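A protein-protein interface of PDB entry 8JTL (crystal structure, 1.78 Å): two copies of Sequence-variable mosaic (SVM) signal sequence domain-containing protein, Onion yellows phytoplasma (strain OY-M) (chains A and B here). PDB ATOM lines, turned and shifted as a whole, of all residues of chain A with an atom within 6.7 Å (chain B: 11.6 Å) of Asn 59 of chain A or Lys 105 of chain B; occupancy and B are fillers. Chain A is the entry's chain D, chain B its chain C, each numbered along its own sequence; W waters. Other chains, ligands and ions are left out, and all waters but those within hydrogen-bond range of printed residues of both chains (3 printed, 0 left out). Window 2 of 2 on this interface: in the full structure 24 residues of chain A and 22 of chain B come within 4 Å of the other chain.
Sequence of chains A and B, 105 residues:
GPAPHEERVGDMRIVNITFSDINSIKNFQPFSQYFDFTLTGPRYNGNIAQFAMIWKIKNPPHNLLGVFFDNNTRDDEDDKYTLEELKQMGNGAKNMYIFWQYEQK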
ATOM      1  N   LYS A  56      -5.142 -12.897  -5.748  1.00  0.00           N
ATOM      2  CA  LYS A  56      -4.802 -13.122  -7.152  1.00  0.00           C
ATOM      3  C   LYS A  56      -5.060 -11.872  -7.970  1.00  0.00           C
ATOM      4  O   LYS A  56      -6.176 -11.324  -7.987  1.00  0.00           O
ATOM      5  CB  LYS A  56      -5.584 -14.313  -7.689  1.00  0.00           C
ATOM      6  CG  LYS A  56      -5.409 -15.511  -6.839  1.00  0.00           C
ATOM      7  CD  LYS A  56      -6.498 -16.559  -7.119  1.00  0.00           C
ATOM      8  CE  LYS A  56      -5.977 -17.994  -6.874  1.00  0.00           C
ATOM      9  NZ  LYS A  56      -7.075 -18.977  -7.192  1.00  0.00           N
ATOM     10  N   ILE A  57      -4.021 -11.418  -8.651  1.00  0.00           N
ATOM     11  CA  ILE A  57      -4.191 -10.325  -9.583  1.00  0.00           C
ATOM     12  C   ILE A  57      -4.965 -10.833 -10.783  1.00  0.00           C
ATOM     13  O   ILE A  57      -4.714 -11.939 -11.290  1.00  0.00           O
ATOM     14  CB  ILE A  57      -2.814  -9.774  -9.975  1.00  0.00           C
ATOM     15  CG1 ILE A  57      -2.145  -9.257  -8.693  1.00  0.00           C
ATOM     16  CG2 ILE A  57      -2.903  -8.674 -11.057  1.00  0.00           C
ATOM     17  CD1 ILE A  57      -0.671  -9.045  -8.834  1.00  0.00           C
ATOM     18  N   LYS A  58      -5.893 -10.022 -11.251  1.00  0.00           N
ATOM     19  CA  LYS A  58      -6.776 -10.418 -12.328  1.00  0.00           C
ATOM     20  C   LYS A  58      -6.038 -10.323 -13.657  1.00  0.00           C
ATOM     21  O   LYS A  58      -5.383  -9.314 -13.924  1.00  0.00           O
ATOM     22  CB  LYS A  58      -7.998  -9.506 -12.340  1.00  0.00           C
ATOM     23  CG  LYS A  58      -9.036  -9.919 -13.366  1.00  0.00           C
ATOM     24  CD  LYS A  58     -10.063  -8.811 -13.560  1.00  0.00           C
ATOM     25  CE  LYS A  58     -11.169  -9.285 -14.530  1.00  0.00           C
ATOM     26  NZ  LYS A  58     -11.473 -10.717 -14.255  1.00  0.00           N
ATOM     27  N   ASN A  59      -6.177 -11.362 -14.503  1.00  0.00           N
ATOM     28  CA  ASN A  59      -5.587 -11.405 -15.848  1.00  0.00           C
ATOM     29  C   ASN A  59      -4.175 -10.853 -15.894  1.00  0.00           C
ATOM     30  O   ASN A  59      -3.888  -9.925 -16.664  1.00  0.00           O
ATOM     31  CB  ASN A  59      -6.426 -10.612 -16.833  1.00  0.00           C
ATOM     32  CG  ASN A  59      -7.807 -11.135 -16.916  1.00  0.00           C
ATOM     33  OD1 ASN A  59      -8.031 -12.346 -16.746  1.00  0.00           O
ATOM     34  ND2 ASN A  59      -8.755 -10.248 -17.178  1.00  0.00           N
ATOM     35  N   PRO A  60      -3.287 -11.381 -15.057  1.00  0.00           N
ATOM     36  CA  PRO A  60      -1.963 -10.815 -14.962  1.00  0.00           C
ATOM     37  C   PRO A  60      -1.196 -11.022 -16.252  1.00  0.00           C
ATOM     38  O   PRO A  60      -1.403 -12.022 -16.959  1.00  0.00           O
ATOM     39  CB  PRO A  60      -1.327 -11.604 -13.811  1.00  0.00           C
ATOM     40  CG  PRO A  60      -1.962 -12.925 -13.894  1.00  0.00           C
ATOM     41  CD  PRO A  60      -3.436 -12.598 -14.237  1.00  0.00           C
ATOM     42  N   PRO A  61      -0.301 -10.101 -16.595  1.00  0.00           N
ATOM     43  CA  PRO A  61       0.663 -10.359 -17.654  1.00  0.00           C
ATOM     44  C   PRO A  61       1.384 -11.641 -17.314  1.00  0.00           C
ATOM     45  O   PRO A  61       1.594 -11.964 -16.138  1.00  0.00           O
ATOM     46  CB  PRO A  61       1.606  -9.153 -17.584  1.00  0.00           C
ATOM     47  CG  PRO A  61       0.844  -8.078 -16.918  1.00  0.00           C
ATOM     48  CD  PRO A  61      -0.067  -8.819 -15.923  1.00  0.00           C
ATOM     49  N   HIS A  62       1.739 -12.381 -18.347  1.00  0.00           N
ATOM     50  CA  HIS A  62       2.368 -13.673 -18.116  1.00  0.00           C
ATOM     51  C   HIS A  62       3.658 -13.514 -17.305  1.00  0.00           C
ATOM     52  O   HIS A  62       4.056 -14.431 -16.581  1.00  0.00           O
ATOM     53  CB  HIS A  62       2.607 -14.333 -19.485  1.00  0.00           C
ATOM     54  CG  HIS A  62       3.702 -15.346 -19.507  1.00  0.00           C
ATOM     55  ND1 HIS A  62       5.032 -15.026 -19.364  1.00  0.00           N
ATOM     56  CD2 HIS A  62       3.653 -16.692 -19.675  1.00  0.00           C
ATOM     57  CE1 HIS A  62       5.757 -16.132 -19.425  1.00  0.00           C
ATOM     58  NE2 HIS A  62       4.947 -17.155 -19.621  1.00  0.00           N
ATOM     59  N   LEU A  64       4.159 -11.240 -14.930  1.00  0.00           N
ATOM     60  CA  LEU A  64       3.955 -10.591 -13.638  1.00  0.00           C
ATOM     61  C   LEU A  64       4.153 -11.617 -12.529  1.00  0.00           C
ATOM     62  O   LEU A  64       3.563 -12.692 -12.555  1.00  0.00           O
ATOM     63  CB  LEU A  64       2.554  -9.981 -13.563  1.00  0.00           C
ATOM     64  CG  LEU A  64       2.311  -9.330 -12.201  1.00  0.00           C
ATOM     65  CD1 LEU A  64       3.248  -8.221 -12.039  1.00  0.00           C
ATOM     66  CD2 LEU A  64       0.845  -8.884 -12.084  1.00  0.00           C
ATOM     67  N   ASP A  79      -8.798 -12.256  -8.335  1.00  0.00           N
ATOM     68  CA  ASP A  79      -9.283 -12.235  -9.697  1.00  0.00           C
ATOM     69  C   ASP A  79     -10.235 -11.076  -9.955  1.00  0.00           C
ATOM     70  O   ASP A  79     -11.188 -11.185 -10.722  1.00  0.00           O
ATOM     71  CB  ASP A  79      -9.909 -13.575 -10.058  1.00  0.00           C
ATOM     72  CG  ASP A  79      -8.893 -14.678  -9.992  1.00  0.00           C
ATOM     73  OD1 ASP A  79      -7.831 -14.487 -10.648  1.00  0.00           O
ATOM     74  OD2 ASP A  79      -9.153 -15.714  -9.359  1.00  0.00           O
ATOM     75  N   LYS A  80      -9.964  -9.957  -9.325  1.00  0.00           N
ATOM     76  CA  LYS A  80     -10.781  -8.771  -9.488  1.00  0.00           C
ATOM     77  C   LYS A  80      -9.976  -7.615 -10.039  1.00  0.00           C
ATOM     78  O   LYS A  80     -10.386  -6.947 -10.995  1.00  0.00           O
ATOM     79  CB  LYS A  80     -11.352  -8.363  -8.137  1.00  0.00           C
ATOM     80  CG  LYS A  80     -12.171  -7.084  -8.197  1.00  0.00           C
ATOM     81  CD  LYS A  80     -13.356  -7.252  -7.332  1.00  0.00           C
ATOM     82  CE  LYS A  80     -14.025  -5.924  -7.093  1.00  0.00           C
ATOM     83  NZ  LYS A  80     -15.034  -6.082  -6.019  1.00  0.00           N
ATOM     84  N   TYR A  81      -8.824  -7.355  -9.428  1.00  0.00           N
ATOM     85  CA  TYR A  81      -8.035  -6.185  -9.734  1.00  0.00           C
ATOM     86  C   TYR A  81      -6.923  -6.586 -10.672  1.00  0.00           C
ATOM     87  O   TYR A  81      -6.069  -7.420 -10.329  1.00  0.00           O
ATOM     88  CB  TYR A  81      -7.467  -5.575  -8.463  1.00  0.00           C
ATOM     89  CG  TYR A  81      -8.602  -5.302  -7.532  1.00  0.00           C
ATOM     90  CD1 TYR A  81      -9.531  -4.325  -7.840  1.00  0.00           C
ATOM     91  CD2 TYR A  81      -8.767  -6.038  -6.372  1.00  0.00           C
ATOM     92  CE1 TYR A  81     -10.564  -4.078  -7.012  1.00  0.00           C
ATOM     93  CE2 TYR A  81      -9.815  -5.806  -5.539  1.00  0.00           C
ATOM     94  CZ  TYR A  81     -10.730  -4.823  -5.887  1.00  0.00           C
ATOM     95  OH  TYR A  81     -11.790  -4.559  -5.073  1.00  0.00           O
ATOM     96  N   THR A  82      -6.946  -5.996 -11.853  1.00  0.00           N
ATOM     97  CA  THR A  82      -5.813  -6.123 -12.728  1.00  0.00           C
ATOM     98  C   THR A  82      -4.632  -5.332 -12.164  1.00  0.00           C
ATOM     99  O   THR A  82      -4.753  -4.496 -11.261  1.00  0.00           O
ATOM    100  CB  THR A  82      -6.145  -5.595 -14.112  1.00  0.00           C
ATOM    101  OG1 THR A  82      -6.507  -4.222 -13.957  1.00  0.00           O
ATOM    102  CG2 THR A  82      -7.293  -6.358 -14.677  1.00  0.00           C
ATOM    103  N   LEU A  83      -3.468  -5.610 -12.729  1.00  0.00           N
ATOM    104  CA  LEU A  83      -2.275  -4.875 -12.332  1.00  0.00           C
ATOM    105  C   LEU A  83      -2.483  -3.378 -12.549  1.00  0.00           C
ATOM    106  O   LEU A  83      -2.106  -2.548 -11.716  1.00  0.00           O
ATOM    107  CB  LEU A  83      -1.107  -5.394 -13.172  1.00  0.00           C
ATOM    108  CG  LEU A  83       0.167  -4.607 -13.014  1.00  0.00           C
ATOM    109  CD1 LEU A  83       0.511  -4.775 -11.492  1.00  0.00           C
ATOM    110  CD2 LEU A  83       1.190  -5.226 -13.864  1.00  0.00           C
ATOM    111  N   THR B  18      -2.580  -1.004 -24.034  1.00  0.00           N
ATOM    112  CA  THR B  18      -2.844  -2.427 -23.958  1.00  0.00           C
ATOM    113  C   THR B  18      -4.049  -2.752 -24.815  1.00  0.00           C
ATOM    114  O   THR B  18      -5.095  -2.111 -24.685  1.00  0.00           O
ATOM    115  CB  THR B  18      -3.079  -2.859 -22.508  1.00  0.00           C
ATOM    116  OG1 THR B  18      -1.897  -2.579 -21.753  1.00  0.00           O
ATOM    117  CG2 THR B  18      -3.359  -4.350 -22.445  1.00  0.00           C
ATOM    118  N   PHE B  19      -3.891  -3.722 -25.703  1.00  0.00           N
ATOM    119  CA  PHE B  19      -4.992  -4.220 -26.507  1.00  0.00           C
ATOM    120  C   PHE B  19      -5.137  -5.712 -26.315  1.00  0.00           C
ATOM    121  O   PHE B  19      -4.148  -6.420 -26.145  1.00  0.00           O
ATOM    122  CB  PHE B  19      -4.749  -3.989 -27.971  1.00  0.00           C
ATOM    123  CG  PHE B  19      -4.903  -2.580 -28.378  1.00  0.00           C
ATOM    124  CD1 PHE B  19      -6.140  -2.084 -28.677  1.00  0.00           C
ATOM    125  CD2 PHE B  19      -3.806  -1.749 -28.409  1.00  0.00           C
ATOM    126  CE1 PHE B  19      -6.294  -0.767 -29.074  1.00  0.00           C
ATOM    127  CE2 PHE B  19      -3.941  -0.434 -28.821  1.00  0.00           C
ATOM    128  CZ  PHE B  19      -5.198   0.052 -29.135  1.00  0.00           C
ATOM    129  N   SER B  20      -6.375  -6.194 -26.428  1.00  0.00           N
ATOM    130  CA  SER B  20      -6.586  -7.634 -26.359  1.00  0.00           C
ATOM    131  C   SER B  20      -6.016  -8.326 -27.589  1.00  0.00           C
ATOM    132  O   SER B  20      -5.431  -9.405 -27.487  1.00  0.00           O
ATOM    133  CB  SER B  20      -8.077  -7.938 -26.243  1.00  0.00           C
ATOM    134  OG  SER B  20      -8.573  -7.379 -25.053  1.00  0.00           O
ATOM    135  N   ASP B  21      -6.189  -7.730 -28.742  1.00  0.00           N
ATOM    136  CA  ASP B  21      -5.663  -8.319 -29.950  1.00  0.00           C
ATOM    137  C   ASP B  21      -4.814  -7.379 -30.749  1.00  0.00           C
ATOM    138  O   ASP B  21      -5.142  -6.227 -30.904  1.00  0.00           O
ATOM    139  CB  ASP B  21      -6.736  -8.964 -30.811  1.00  0.00           C
ATOM    140  CG  ASP B  21      -8.028  -8.243 -30.781  1.00  0.00           C
ATOM    141  OD1 ASP B  21      -8.170  -7.324 -31.588  1.00  0.00           O
ATOM    142  OD2 ASP B  21      -8.917  -8.624 -29.994  1.00  0.00           O
ATOM    143  N   HIS B  62       6.388 -11.486 -22.727  1.00  0.00           N
ATOM    144  CA  HIS B  62       5.502 -12.237 -23.622  1.00  0.00           C
ATOM    145  C   HIS B  62       4.371 -11.377 -24.176  1.00  0.00           C
ATOM    146  O   HIS B  62       3.969 -11.562 -25.322  1.00  0.00           O
ATOM    147  CB  HIS B  62       4.925 -13.464 -22.894  1.00  0.00           C
ATOM    148  CG  HIS B  62       3.972 -14.292 -23.709  1.00  0.00           C
ATOM    149  ND1 HIS B  62       2.716 -14.631 -23.240  1.00  0.00           N
ATOM    150  CD2 HIS B  62       4.069 -14.847 -24.943  1.00  0.00           C
ATOM    151  CE1 HIS B  62       2.077 -15.342 -24.150  1.00  0.00           C
ATOM    152  NE2 HIS B  62       2.874 -15.486 -25.192  1.00  0.00           N
ATOM    153  N   ASN B  63       3.849 -10.433 -23.401  1.00  0.00           N
ATOM    154  CA  ASN B  63       2.739  -9.631 -23.903  1.00  0.00           C
ATOM    155  C   ASN B  63       3.169  -8.278 -24.459  1.00  0.00           C
ATOM    156  O   ASN B  63       2.297  -7.462 -24.767  1.00  0.00           O
ATOM    157  CB  ASN B  63       1.672  -9.418 -22.823  1.00  0.00           C
ATOM    158  CG  ASN B  63       2.128  -8.486 -21.757  1.00  0.00           C
ATOM    159  OD1 ASN B  63       3.311  -8.490 -21.392  1.00  0.00           O
ATOM    160  ND2 ASN B  63       1.219  -7.648 -21.265  1.00  0.00           N
ATOM    161  N   TRP B 100       1.053  -3.274 -25.423  1.00  0.00           N
ATOM    162  CA  TRP B 100       0.971  -4.503 -24.661  1.00  0.00           C
ATOM    163  C   TRP B 100      -0.245  -5.256 -25.121  1.00  0.00           C
ATOM    164  O   TRP B 100      -1.249  -4.653 -25.516  1.00  0.00           O
ATOM    165  CB  TRP B 100       0.808  -4.221 -23.201  1.00  0.00           C
ATOM    166  CG  TRP B 100       1.892  -3.489 -22.659  1.00  0.00           C
ATOM    167  CD1 TRP B 100       1.946  -2.157 -22.429  1.00  0.00           C
ATOM    168  CD2 TRP B 100       3.138  -4.034 -22.238  1.00  0.00           C
ATOM    169  NE1 TRP B 100       3.136  -1.837 -21.825  1.00  0.00           N
ATOM    170  CE2 TRP B 100       3.889  -2.978 -21.707  1.00  0.00           C
ATOM    171  CE3 TRP B 100       3.667  -5.333 -22.206  1.00  0.00           C
ATOM    172  CZ2 TRP B 100       5.158  -3.164 -21.178  1.00  0.00           C
ATOM    173  CZ3 TRP B 100       4.923  -5.515 -21.682  1.00  0.00           C
ATOM    174  CH2 TRP B 100       5.653  -4.438 -21.170  1.00  0.00           C
ATOM    175  N   GLN B 101      -0.174  -6.572 -25.033  1.00  0.00           N
ATOM    176  CA  GLN B 101      -1.348  -7.389 -25.271  1.00  0.00           C
ATOM    177  C   GLN B 101      -1.970  -7.746 -23.931  1.00  0.00           C
ATOM    178  O   GLN B 101      -1.274  -8.155 -22.991  1.00  0.00           O
ATOM    179  CB  GLN B 101      -1.013  -8.661 -26.032  1.00  0.00           C
ATOM    180  CG  GLN B 101      -2.247  -9.512 -26.360  1.00  0.00           C
ATOM    181  CD  GLN B 101      -2.036 -10.277 -27.624  1.00  0.00           C
ATOM    182  OE1 GLN B 101      -0.925 -10.714 -27.901  1.00  0.00           O
ATOM    183  NE2 GLN B 101      -3.099 -10.475 -28.392  1.00  0.00           N
ATOM    184  N   TYR B 102      -3.267  -7.514 -23.821  1.00  0.00           N
ATOM    185  CA  TYR B 102      -3.975  -7.965 -22.639  1.00  0.00           C
ATOM    186  C   TYR B 102      -3.917  -9.488 -22.582  1.00  0.00           C
ATOM    187  O   TYR B 102      -4.053 -10.153 -23.604  1.00  0.00           O
ATOM    188  CB  TYR B 102      -5.402  -7.438 -22.721  1.00  0.00           C
ATOM    189  CG  TYR B 102      -6.143  -7.513 -21.414  1.00  0.00           C
ATOM    190  CD1 TYR B 102      -6.616  -8.737 -20.969  1.00  0.00           C
ATOM    191  CD2 TYR B 102      -6.337  -6.385 -20.622  1.00  0.00           C
ATOM    192  CE1 TYR B 102      -7.272  -8.839 -19.826  1.00  0.00           C
ATOM    193  CE2 TYR B 102      -7.038  -6.482 -19.417  1.00  0.00           C
ATOM    194  CZ  TYR B 102      -7.501  -7.718 -19.050  1.00  0.00           C
ATOM    195  OH  TYR B 102      -8.217  -7.890 -17.901  1.00  0.00           O
ATOM    196  N   GLU B 103      -3.634 -10.043 -21.413  1.00  0.00           N
ATOM    197  CA  GLU B 103      -3.546 -11.492 -21.281  1.00  0.00           C
ATOM    198  C   GLU B 103      -4.798 -11.953 -20.560  1.00  0.00           C
ATOM    199  O   GLU B 103      -4.962 -11.694 -19.360  1.00  0.00           O
ATOM    200  CB  GLU B 103      -2.289 -11.926 -20.544  1.00  0.00           C
ATOM    201  CG  GLU B 103      -1.053 -11.174 -20.989  1.00  0.00           C
ATOM    202  CD  GLU B 103       0.112 -12.101 -21.168  1.00  0.00           C
ATOM    203  OE1 GLU B 103      -0.105 -13.183 -21.759  1.00  0.00           O
ATOM    204  OE2 GLU B 103       1.224 -11.773 -20.678  1.00  0.00           O
ATOM    205  N   GLN B 104      -5.678 -12.614 -21.297  1.00  0.00           N
ATOM    206  CA  GLN B 104      -6.945 -13.089 -20.767  1.00  0.00           C
ATOM    207  C   GLN B 104      -6.877 -14.587 -20.456  1.00  0.00           C
ATOM    208  O   GLN B 104      -5.836 -15.238 -20.598  1.00  0.00           O
ATOM    209  CB  GLN B 104      -8.089 -12.773 -21.739  1.00  0.00           C
ATOM    210  CG  GLN B 104      -7.774 -12.935 -23.246  1.00  0.00           C
ATOM    211  CD  GLN B 104      -8.426 -11.845 -24.125  1.00  0.00           C
ATOM    212  OE1 GLN B 104      -8.586 -10.691 -23.710  1.00  0.00           O
ATOM    213  NE2 GLN B 104      -8.820 -12.229 -25.339  1.00  0.00           N
ATOM    214  N   LYS B 105      -8.017 -15.132 -20.030  1.00  0.00           N
ATOM    215  CA  LYS B 105      -8.140 -16.531 -19.621  1.00  0.00           C
ATOM    216  C   LYS B 105      -7.211 -16.841 -18.446  1.00  0.00           C
ATOM    217  O   LYS B 105      -6.792 -15.939 -17.717  1.00  0.00           O
ATOM    218  CB  LYS B 105      -7.841 -17.474 -20.793  1.00  0.00           C
ATOM    219  CG  LYS B 105      -8.543 -17.115 -22.092  1.00  0.00           C
ATOM    220  CD  LYS B 105      -8.094 -18.034 -23.212  1.00  0.00           C
ATOM    221  CE  LYS B 105      -6.830 -17.482 -23.873  1.00  0.00           C
ATOM    222  NZ  LYS B 105      -5.566 -17.839 -23.148  1.00  0.00           N
HETATM  223  O   HOH W   1      -3.526 -13.458 -17.356  1.00  0.00           O
HETATM  224  O   HOH W   2       3.591 -10.777 -20.013  1.00  0.00           O
HETATM  225  O   HOH W   3      -3.045  -8.584 -18.916  1.00  0.00           O
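The backbone carbonyl oxygen (O) of Phe 19 of chain B sits at hydrogen-bond distance from the backbone NH (N) of Tyr 102 of chain B (2.7 Å). A ring nitrogen (ND1) of His 62 of chain B is in hydrogen-bond range of the side-chain carboxylate (OE1) of Glu 103 of chain B (3.5 Å). N of Gln 101 of chain B lies within hydrogen-bond range of O of Asn 63 of chain B (2.6 Å).
Asn 59 of chain A touches just these residues of chain B: Tyr 102, Glu 103 and Lys 105. Lys 105 of chain B touches just one residue of chain A: Asn 59. No residue of chain B comes within 4 Å of Lys 58 of chain A. Of chain B, only Glu 103 comes within 4 Å of Pro 60 of chain A. Asp 79 of chain A touches none of the printed residues of chain B. Printed residues of chain A within 4 Å of His 62 of chain B: His 62. Printed residues of chain A within 4 Å of Asn 63 of chain B: Pro 61. Of the printed residues of chain B, Pro 61 of chain A touches Asn 63 and Glu 103. Printed residues of chain B within 4 Å of Thr 82 of chain A: Tyr 102.
ND2 of Asn 59 of chain A is in hydrogen-bond range of OH of Tyr 102 of chain B (2.5 Å). N of His 62 of chain A sits at hydrogen-bond distance from OE2 of Glu 103 of chain B (2.5 Å). O of Asn 59 of chain A sits close to O of Glu 103 of chain B (3.4 Å).
Of the 12 printed residues of chain B, 5 touch a printed residue of chain A. Among the printed residues, no Asp or Glu carboxylate lies within 4 Å of a Lys or Arg side-chain nitrogen of the other chain.
Asn 59 of chain A touches Lys 105 of chain B. Pro 60 of chain A touches Glu 103 of chain B. CB of Pro 61 of chain A touches ND2 of Asn 63 of chain B (3.996 Å). C of Pro 61 of chain A touches OE2 of Glu 103 of chain B, at 3.4 Å. CB of His 62 of chain A touches ND1 of His 62 of chain B, 3.8 Å away. CG2 of Thr 82 of chain A touches OH of Tyr 102 of chain B, at 3.7 Å.
His 62 of chain A touches its own counterpart, His 62 of chain B. Of the 9 pairs that touch across the chains among the printed residues, 1 has its exchanged pair printed and touching as well.
Water W1 lies within hydrogen-bond range of the backbone carbonyl oxygen of Pro 60 of chain A and the backbone carbonyl oxygen of Glu 103 of chain B. Water W2 lies within hydrogen-bond range of OE2 of Glu 103 of chain B, OD1 of Asn 63 of chain B and N of His 62 of chain A. Water W3 lies within hydrogen-bond range of the backbone carbonyl oxygen of Asn 59 of chain A (2.8 Å) and the backbone NH of Glu 103 of chain B (3.0 Å).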
